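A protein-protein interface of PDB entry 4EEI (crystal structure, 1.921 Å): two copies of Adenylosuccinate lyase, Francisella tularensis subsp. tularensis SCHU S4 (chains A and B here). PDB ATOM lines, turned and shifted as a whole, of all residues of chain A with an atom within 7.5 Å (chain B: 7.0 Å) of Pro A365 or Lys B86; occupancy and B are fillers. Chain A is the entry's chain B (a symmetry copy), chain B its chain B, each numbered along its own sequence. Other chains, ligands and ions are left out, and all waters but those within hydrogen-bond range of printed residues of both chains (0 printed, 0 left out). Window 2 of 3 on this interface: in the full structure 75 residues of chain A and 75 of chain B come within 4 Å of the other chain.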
ATOM      1  N   LEU A 360      12.918  -1.477   2.492  1.00  0.00           N
ATOM      2  CA  LEU A 360      11.697  -1.705   1.723  1.00  0.00           C
ATOM      3  C   LEU A 360      10.776  -0.493   1.797  1.00  0.00           C
ATOM      4  O   LEU A 360      10.171  -0.096   0.797  1.00  0.00           O
ATOM      5  CB  LEU A 360      10.967  -2.957   2.213  1.00  0.00           C
ATOM      6  CG  LEU A 360      11.686  -4.293   2.012  1.00  0.00           C
ATOM      7  CD1 LEU A 360      10.829  -5.444   2.508  1.00  0.00           C
ATOM      8  CD2 LEU A 360      12.037  -4.489   0.552  1.00  0.00           C
ATOM      9  N   VAL A 361      10.678   0.091   2.988  1.00  0.00           N
ATOM     10  CA  VAL A 361       9.873   1.291   3.187  1.00  0.00           C
ATOM     11  C   VAL A 361      10.352   2.402   2.255  1.00  0.00           C
ATOM     12  O   VAL A 361       9.557   3.021   1.551  1.00  0.00           O
ATOM     13  CB  VAL A 361       9.936   1.765   4.655  1.00  0.00           C
ATOM     14  CG1 VAL A 361       9.369   3.174   4.797  1.00  0.00           C
ATOM     15  CG2 VAL A 361       9.183   0.798   5.559  1.00  0.00           C
ATOM     16  N   ALA A 362      11.664   2.627   2.236  1.00  0.00           N
ATOM     17  CA  ALA A 362      12.251   3.704   1.438  1.00  0.00           C
ATOM     18  C   ALA A 362      12.249   3.446  -0.073  1.00  0.00           C
ATOM     19  O   ALA A 362      12.356   4.388  -0.862  1.00  0.00           O
ATOM     20  CB  ALA A 362      13.649   3.995   1.908  1.00  0.00           C
ATOM     21  N   ASN A 363      12.135   2.182  -0.474  1.00  0.00           N
ATOM     22  CA  ASN A 363      12.296   1.836  -1.887  1.00  0.00           C
ATOM     23  C   ASN A 363      11.100   1.172  -2.565  1.00  0.00           C
ATOM     24  O   ASN A 363      11.144   0.895  -3.761  1.00  0.00           O
ATOM     25  CB  ASN A 363      13.557   0.990  -2.090  1.00  0.00           C
ATOM     26  CG  ASN A 363      14.827   1.781  -1.857  1.00  0.00           C
ATOM     27  OD1 ASN A 363      15.184   2.647  -2.656  1.00  0.00           O
ATOM     28  ND2 ASN A 363      15.518   1.491  -0.757  1.00  0.00           N
ATOM     29  N   THR A 364      10.044   0.907  -1.805  1.00  0.00           N
ATOM     30  CA  THR A 364       8.811   0.384  -2.382  1.00  0.00           C
ATOM     31  C   THR A 364       7.663   1.322  -2.045  1.00  0.00           C
ATOM     32  O   THR A 364       7.759   2.100  -1.099  1.00  0.00           O
ATOM     33  CB  THR A 364       8.460  -1.022  -1.850  1.00  0.00           C
ATOM     34  OG1 THR A 364       7.933  -0.919  -0.521  1.00  0.00           O
ATOM     35  CG2 THR A 364       9.683  -1.923  -1.847  1.00  0.00           C
ATOM     36  N   PRO A 365       6.583   1.265  -2.838  1.00  0.00           N
ATOM     37  CA  PRO A 365       5.301   1.911  -2.533  1.00  0.00           C
ATOM     38  C   PRO A 365       4.546   1.240  -1.377  1.00  0.00           C
ATOM     39  O   PRO A 365       3.551   1.796  -0.911  1.00  0.00           O
ATOM     40  CB  PRO A 365       4.506   1.735  -3.834  1.00  0.00           C
ATOM     41  CG  PRO A 365       5.534   1.571  -4.896  1.00  0.00           C
ATOM     42  CD  PRO A 365       6.660   0.830  -4.245  1.00  0.00           C
ATOM     43  N   PHE A 366       4.999   0.069  -0.934  1.00  0.00           N
ATOM     44  CA  PHE A 366       4.357  -0.655   0.168  1.00  0.00           C
ATOM     45  C   PHE A 366       4.380   0.143   1.476  1.00  0.00           C
ATOM     46  O   PHE A 366       5.195   1.047   1.635  1.00  0.00           O
ATOM     47  CB  PHE A 366       5.048  -2.003   0.383  1.00  0.00           C
ATOM     48  CG  PHE A 366       4.280  -3.178  -0.160  1.00  0.00           C
ATOM     49  CD1 PHE A 366       2.903  -3.256  -0.002  1.00  0.00           C
ATOM     50  CD2 PHE A 366       4.933  -4.209  -0.824  1.00  0.00           C
ATOM     51  CE1 PHE A 366       2.191  -4.338  -0.496  1.00  0.00           C
ATOM     52  CE2 PHE A 366       4.227  -5.294  -1.322  1.00  0.00           C
ATOM     53  CZ  PHE A 366       2.855  -5.358  -1.156  1.00  0.00           C
ATOM     54  N   MET A 367       3.495  -0.190   2.413  1.00  0.00           N
ATOM     55  CA  MET A 367       3.511   0.482   3.713  1.00  0.00           C
ATOM     56  C   MET A 367       4.130  -0.390   4.811  1.00  0.00           C
ATOM     57  O   MET A 367       4.219  -1.610   4.667  1.00  0.00           O
ATOM     58  CB  MET A 367       2.124   1.007   4.108  1.00  0.00           C
ATOM     59  CG  MET A 367       2.068   2.528   4.305  1.00  0.00           C
ATOM     60  SD  MET A 367       1.884   3.494   2.787  1.00  0.00           S
ATOM     61  CE  MET A 367       0.231   3.017   2.294  1.00  0.00           C
ATOM     62  N   ARG A 368       4.521   0.257   5.904  1.00  0.00           N
ATOM     63  CA  ARG A 368       5.343  -0.359   6.938  1.00  0.00           C
ATOM     64  C   ARG A 368       4.829  -1.737   7.332  1.00  0.00           C
ATOM     65  O   ARG A 368       5.586  -2.705   7.351  1.00  0.00           O
ATOM     66  CB  ARG A 368       5.399   0.547   8.169  1.00  0.00           C
ATOM     67  CG  ARG A 368       6.521   0.227   9.142  1.00  0.00           C
ATOM     68  CD  ARG A 368       6.525   1.213  10.300  1.00  0.00           C
ATOM     69  NE  ARG A 368       7.589   0.936  11.260  1.00  0.00           N
ATOM     70  CZ  ARG A 368       7.521  -0.001  12.199  1.00  0.00           C
ATOM     71  NH1 ARG A 368       8.536  -0.183  13.031  1.00  0.00           N
ATOM     72  NH2 ARG A 368       6.438  -0.759  12.305  1.00  0.00           N
ATOM     73  N   ASP A 370       2.991  -3.876   5.885  1.00  0.00           N
ATOM     74  CA  ASP A 370       3.235  -4.839   4.812  1.00  0.00           C
ATOM     75  C   ASP A 370       4.705  -5.263   4.737  1.00  0.00           C
ATOM     76  O   ASP A 370       5.014  -6.455   4.720  1.00  0.00           O
ATOM     77  CB  ASP A 370       2.799  -4.262   3.463  1.00  0.00           C
ATOM     78  CG  ASP A 370       1.325  -4.491   3.175  1.00  0.00           C
ATOM     79  OD1 ASP A 370       0.781  -5.520   3.633  1.00  0.00           O
ATOM     80  OD2 ASP A 370       0.716  -3.644   2.484  1.00  0.00           O
ATOM     81  N   CYS A 371       5.602  -4.280   4.686  1.00  0.00           N
ATOM     82  CA  CYS A 371       7.036  -4.540   4.572  1.00  0.00           C
ATOM     83  C   CYS A 371       7.550  -5.395   5.727  1.00  0.00           C
ATOM     84  O   CYS A 371       8.474  -6.193   5.557  1.00  0.00           O
ATOM     85  CB  CYS A 371       7.820  -3.227   4.534  1.00  0.00           C
ATOM     86  SG  CYS A 371       7.443  -2.118   3.162  1.00  0.00           S
ATOM     87  N   ILE A 402       8.763  -6.158  -8.268  1.00  0.00           N
ATOM     88  CA  ILE A 402       9.545  -4.962  -7.964  1.00  0.00           C
ATOM     89  C   ILE A 402      11.051  -5.165  -8.177  1.00  0.00           C
ATOM     90  O   ILE A 402      11.621  -6.181  -7.769  1.00  0.00           O
ATOM     91  CB  ILE A 402       9.254  -4.459  -6.521  1.00  0.00           C
ATOM     92  CG1 ILE A 402       7.801  -3.997  -6.410  1.00  0.00           C
ATOM     93  CG2 ILE A 402      10.202  -3.333  -6.120  1.00  0.00           C
ATOM     94  CD1 ILE A 402       7.434  -3.436  -5.051  1.00  0.00           C
ATOM     95  N   LEU B  31      12.323  15.017   9.319  1.00  0.00           N
ATOM     96  CA  LEU B  31      11.478  14.613   8.194  1.00  0.00           C
ATOM     97  C   LEU B  31      11.678  15.556   7.013  1.00  0.00           C
ATOM     98  O   LEU B  31      11.756  15.119   5.866  1.00  0.00           O
ATOM     99  CB  LEU B  31      10.001  14.568   8.604  1.00  0.00           C
ATOM    100  CG  LEU B  31       8.980  14.117   7.554  1.00  0.00           C
ATOM    101  CD1 LEU B  31       9.226  12.686   7.108  1.00  0.00           C
ATOM    102  CD2 LEU B  31       7.551  14.266   8.088  1.00  0.00           C
ATOM    103  N   THR B  43       5.971  17.021   2.579  1.00  0.00           N
ATOM    104  CA  THR B  43       5.388  16.126   3.575  1.00  0.00           C
ATOM    105  C   THR B  43       5.438  16.714   4.985  1.00  0.00           C
ATOM    106  O   THR B  43       4.431  16.738   5.694  1.00  0.00           O
ATOM    107  CB  THR B  43       6.071  14.747   3.558  1.00  0.00           C
ATOM    108  OG1 THR B  43       5.917  14.153   2.261  1.00  0.00           O
ATOM    109  CG2 THR B  43       5.455  13.837   4.600  1.00  0.00           C
ATOM    110  N   ILE B  47       2.171  17.922   7.507  1.00  0.00           N
ATOM    111  CA  ILE B  47       1.937  17.432   8.858  1.00  0.00           C
ATOM    112  C   ILE B  47       2.010  18.579   9.866  1.00  0.00           C
ATOM    113  O   ILE B  47       1.200  18.660  10.796  1.00  0.00           O
ATOM    114  CB  ILE B  47       2.933  16.308   9.212  1.00  0.00           C
ATOM    115  CG1 ILE B  47       2.723  15.107   8.281  1.00  0.00           C
ATOM    116  CG2 ILE B  47       2.801  15.896  10.674  1.00  0.00           C
ATOM    117  CD1 ILE B  47       3.711  13.959   8.505  1.00  0.00           C
ATOM    118  N   ALA B  77       0.519   9.856  13.728  1.00  0.00           N
ATOM    119  CA  ALA B  77       0.252   9.076  12.521  1.00  0.00           C
ATOM    120  C   ALA B  77      -1.231   8.794  12.278  1.00  0.00           C
ATOM    121  O   ALA B  77      -1.689   8.769  11.126  1.00  0.00           O
ATOM    122  CB  ALA B  77       1.039   7.769  12.556  1.00  0.00           C
ATOM    123  N   THR B  81      -3.303   9.948   6.496  1.00  0.00           N
ATOM    124  CA  THR B  81      -3.318   8.768   5.636  1.00  0.00           C
ATOM    125  C   THR B  81      -2.063   7.938   5.884  1.00  0.00           C
ATOM    126  O   THR B  81      -1.042   8.463   6.339  1.00  0.00           O
ATOM    127  CB  THR B  81      -3.387   9.142   4.135  1.00  0.00           C
ATOM    128  OG1 THR B  81      -2.253   9.946   3.779  1.00  0.00           O
ATOM    129  CG2 THR B  81      -4.661   9.911   3.827  1.00  0.00           C
ATOM    130  N   ALA B  82      -2.139   6.644   5.590  1.00  0.00           N
ATOM    131  CA  ALA B  82      -0.987   5.762   5.748  1.00  0.00           C
ATOM    132  C   ALA B  82       0.182   6.271   4.909  1.00  0.00           C
ATOM    133  O   ALA B  82       1.346   6.169   5.313  1.00  0.00           O
ATOM    134  CB  ALA B  82      -1.349   4.346   5.357  1.00  0.00           C
ATOM    135  N   GLU B  83      -0.142   6.830   3.744  1.00  0.00           N
ATOM    136  CA  GLU B  83       0.861   7.398   2.843  1.00  0.00           C
ATOM    137  C   GLU B  83       1.597   8.593   3.458  1.00  0.00           C
ATOM    138  O   GLU B  83       2.829   8.617   3.513  1.00  0.00           O
ATOM    139  CB  GLU B  83       0.208   7.819   1.523  1.00  0.00           C
ATOM    140  CG  GLU B  83       1.186   8.339   0.479  1.00  0.00           C
ATOM    141  CD  GLU B  83       1.898   7.223  -0.273  1.00  0.00           C
ATOM    142  OE1 GLU B  83       1.272   6.166  -0.507  1.00  0.00           O
ATOM    143  OE2 GLU B  83       3.083   7.406  -0.631  1.00  0.00           O
ATOM    144  N   THR B  84       0.838   9.586   3.910  1.00  0.00           N
ATOM    145  CA  THR B  84       1.417  10.802   4.478  1.00  0.00           C
ATOM    146  C   THR B  84       2.290  10.524   5.701  1.00  0.00           C
ATOM    147  O   THR B  84       3.338  11.147   5.884  1.00  0.00           O
ATOM    148  CB  THR B  84       0.315  11.809   4.855  1.00  0.00           C
ATOM    149  OG1 THR B  84      -0.352  12.241   3.664  1.00  0.00           O
ATOM    150  CG2 THR B  84       0.902  13.019   5.562  1.00  0.00           C
ATOM    151  N   GLY B  85       1.867   9.583   6.536  1.00  0.00           N
ATOM    152  CA  GLY B  85       2.602   9.297   7.755  1.00  0.00           C
ATOM    153  C   GLY B  85       3.707   8.277   7.557  1.00  0.00           C
ATOM    154  O   GLY B  85       4.376   7.897   8.518  1.00  0.00           O
ATOM    155  N   LYS B  86       3.913   7.849   6.313  1.00  0.00           N
ATOM    156  CA  LYS B  86       4.858   6.769   6.023  1.00  0.00           C
ATOM    157  C   LYS B  86       6.283   6.983   6.548  1.00  0.00           C
ATOM    158  O   LYS B  86       6.898   6.062   7.099  1.00  0.00           O
ATOM    159  CB  LYS B  86       4.908   6.489   4.523  1.00  0.00           C
ATOM    160  CG  LYS B  86       5.884   5.395   4.171  1.00  0.00           C
ATOM    161  CD  LYS B  86       5.658   4.845   2.776  1.00  0.00           C
ATOM    162  CE  LYS B  86       6.515   3.614   2.574  1.00  0.00           C
ATOM    163  NZ  LYS B  86       6.348   2.971   1.239  1.00  0.00           N
ATOM    164  N   PHE B  87       6.813   8.187   6.365  1.00  0.00           N
ATOM    165  CA  PHE B  87       8.199   8.441   6.728  1.00  0.00           C
ATOM    166  C   PHE B  87       8.319   9.153   8.066  1.00  0.00           C
ATOM    167  O   PHE B  87       9.398   9.609   8.442  1.00  0.00           O
ATOM    168  CB  PHE B  87       8.913   9.214   5.617  1.00  0.00           C
ATOM    169  CG  PHE B  87       9.143   8.399   4.373  1.00  0.00           C
ATOM    170  CD1 PHE B  87       8.419   8.645   3.214  1.00  0.00           C
ATOM    171  CD2 PHE B  87      10.067   7.370   4.372  1.00  0.00           C
ATOM    172  CE1 PHE B  87       8.628   7.890   2.073  1.00  0.00           C
ATOM    173  CE2 PHE B  87      10.281   6.613   3.239  1.00  0.00           C
ATOM    174  CZ  PHE B  87       9.561   6.870   2.087  1.00  0.00           C
ATOM    175  N   PHE B  88       7.210   9.237   8.791  1.00  0.00           N
ATOM    176  CA  PHE B  88       7.249   9.810  10.127  1.00  0.00           C
ATOM    177  C   PHE B  88       8.101   8.903  11.008  1.00  0.00           C
ATOM    178  O   PHE B  88       7.927   7.681  11.008  1.00  0.00           O
ATOM    179  CB  PHE B  88       5.842   9.970  10.707  1.00  0.00           C
ATOM    180  CG  PHE B  88       5.779  10.905  11.884  1.00  0.00           C
ATOM    181  CD1 PHE B  88       5.795  12.280  11.692  1.00  0.00           C
ATOM    182  CD2 PHE B  88       5.723  10.412  13.183  1.00  0.00           C
ATOM    183  CE1 PHE B  88       5.740  13.154  12.773  1.00  0.00           C
ATOM    184  CE2 PHE B  88       5.667  11.278  14.272  1.00  0.00           C
ATOM    185  CZ  PHE B  88       5.679  12.652  14.066  1.00  0.00           C
ATOM    186  N   HIS B  89       9.047   9.506  11.720  1.00  0.00           N
ATOM    187  CA  HIS B  89       9.951   8.764  12.598  1.00  0.00           C
ATOM    188  C   HIS B  89      10.740   7.700  11.829  1.00  0.00           C
ATOM    189  O   HIS B  89      10.747   6.524  12.190  1.00  0.00           O
ATOM    190  CB  HIS B  89       9.169   8.135  13.752  1.00  0.00           C
ATOM    191  CG  HIS B  89      10.019   7.759  14.923  1.00  0.00           C
ATOM    192  ND1 HIS B  89      10.328   8.647  15.932  1.00  0.00           N
ATOM    193  CD2 HIS B  89      10.624   6.593  15.249  1.00  0.00           C
ATOM    194  CE1 HIS B  89      11.089   8.043  16.829  1.00  0.00           C
ATOM    195  NE2 HIS B  89      11.283   6.796  16.437  1.00  0.00           N
ATOM    196  N   PHE B  90      11.403   8.121  10.762  1.00  0.00           N
ATOM    197  CA  PHE B  90      12.140   7.202   9.919  1.00  0.00           C
ATOM    198  C   PHE B  90      13.628   7.336  10.220  1.00  0.00           C
ATOM    199  O   PHE B  90      14.156   8.448  10.249  1.00  0.00           O
ATOM    200  CB  PHE B  90      11.847   7.531   8.454  1.00  0.00           C
ATOM    201  CG  PHE B  90      12.479   6.594   7.475  1.00  0.00           C
ATOM    202  CD1 PHE B  90      13.711   6.892   6.914  1.00  0.00           C
ATOM    203  CD2 PHE B  90      11.829   5.435   7.084  1.00  0.00           C
ATOM    204  CE1 PHE B  90      14.291   6.044   5.993  1.00  0.00           C
ATOM    205  CE2 PHE B  90      12.408   4.574   6.163  1.00  0.00           C
ATOM    206  CZ  PHE B  90      13.644   4.879   5.616  1.00  0.00           C
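No position is printed for both chains. Of the 9 pairs that touch across the chains among the printed residues, none has its exchanged pair printed and touching as well.
The backbone carbonyl oxygen of Leu A360 lies within hydrogen-bond range of the side-chain hydroxyl of Thr A364 (2.7 Å). The backbone NH (N) of Phe A366 sits at hydrogen-bond distance from the side-chain hydroxyl (OG1) of Thr A364 (3.1 Å). The backbone carbonyl oxygen of Met A367 sits at hydrogen-bond distance from the side-chain sulfur of Cys A371.
Hydrophobic or aromatic side chains of chain A within 4 Å of the printed part of chain B: Val A361, Ala A362 and Met A367.
Val A361 touches Phe B87 (CG1 to CE2, 3.9 Å). Phe B90 touches Val A361. Ala A362 touches Phe B87. Phe B90 touches Ala A362. Pro A365 touches Lys B86.
The backbone carbonyl oxygen of Val A361 is in hydrogen-bond range of the side-chain amino group of Lys B86, at 3.2 Å. The side-chain amino group (NZ) of Lys B86 is in hydrogen-bond range of the backbone carbonyl oxygen (O) of Thr A364 (2.9 Å). NZ of Lys B86 lies close to O of Phe A366 (2.3 Å). The side-chain sulfur (SD) of Met A367 lies close to the backbone carbonyl oxygen (O) of Ala B82, 3.7 Å away.
Pro A365 touches just one residue of chain B: Lys B86. No residue of chain A comes within 4 Å of Gly B85. Of the printed residues of chain B, Ala A362 touches Phe B87 (3.9 Å) and Phe B90 (3.8 Å). Printed residues of chain B within 4 Å of Thr A364: Lys B86 (2.9 Å). The nearest printed residue of chain A that does not touch Lys B86 is Met A367 (4.01 Å).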
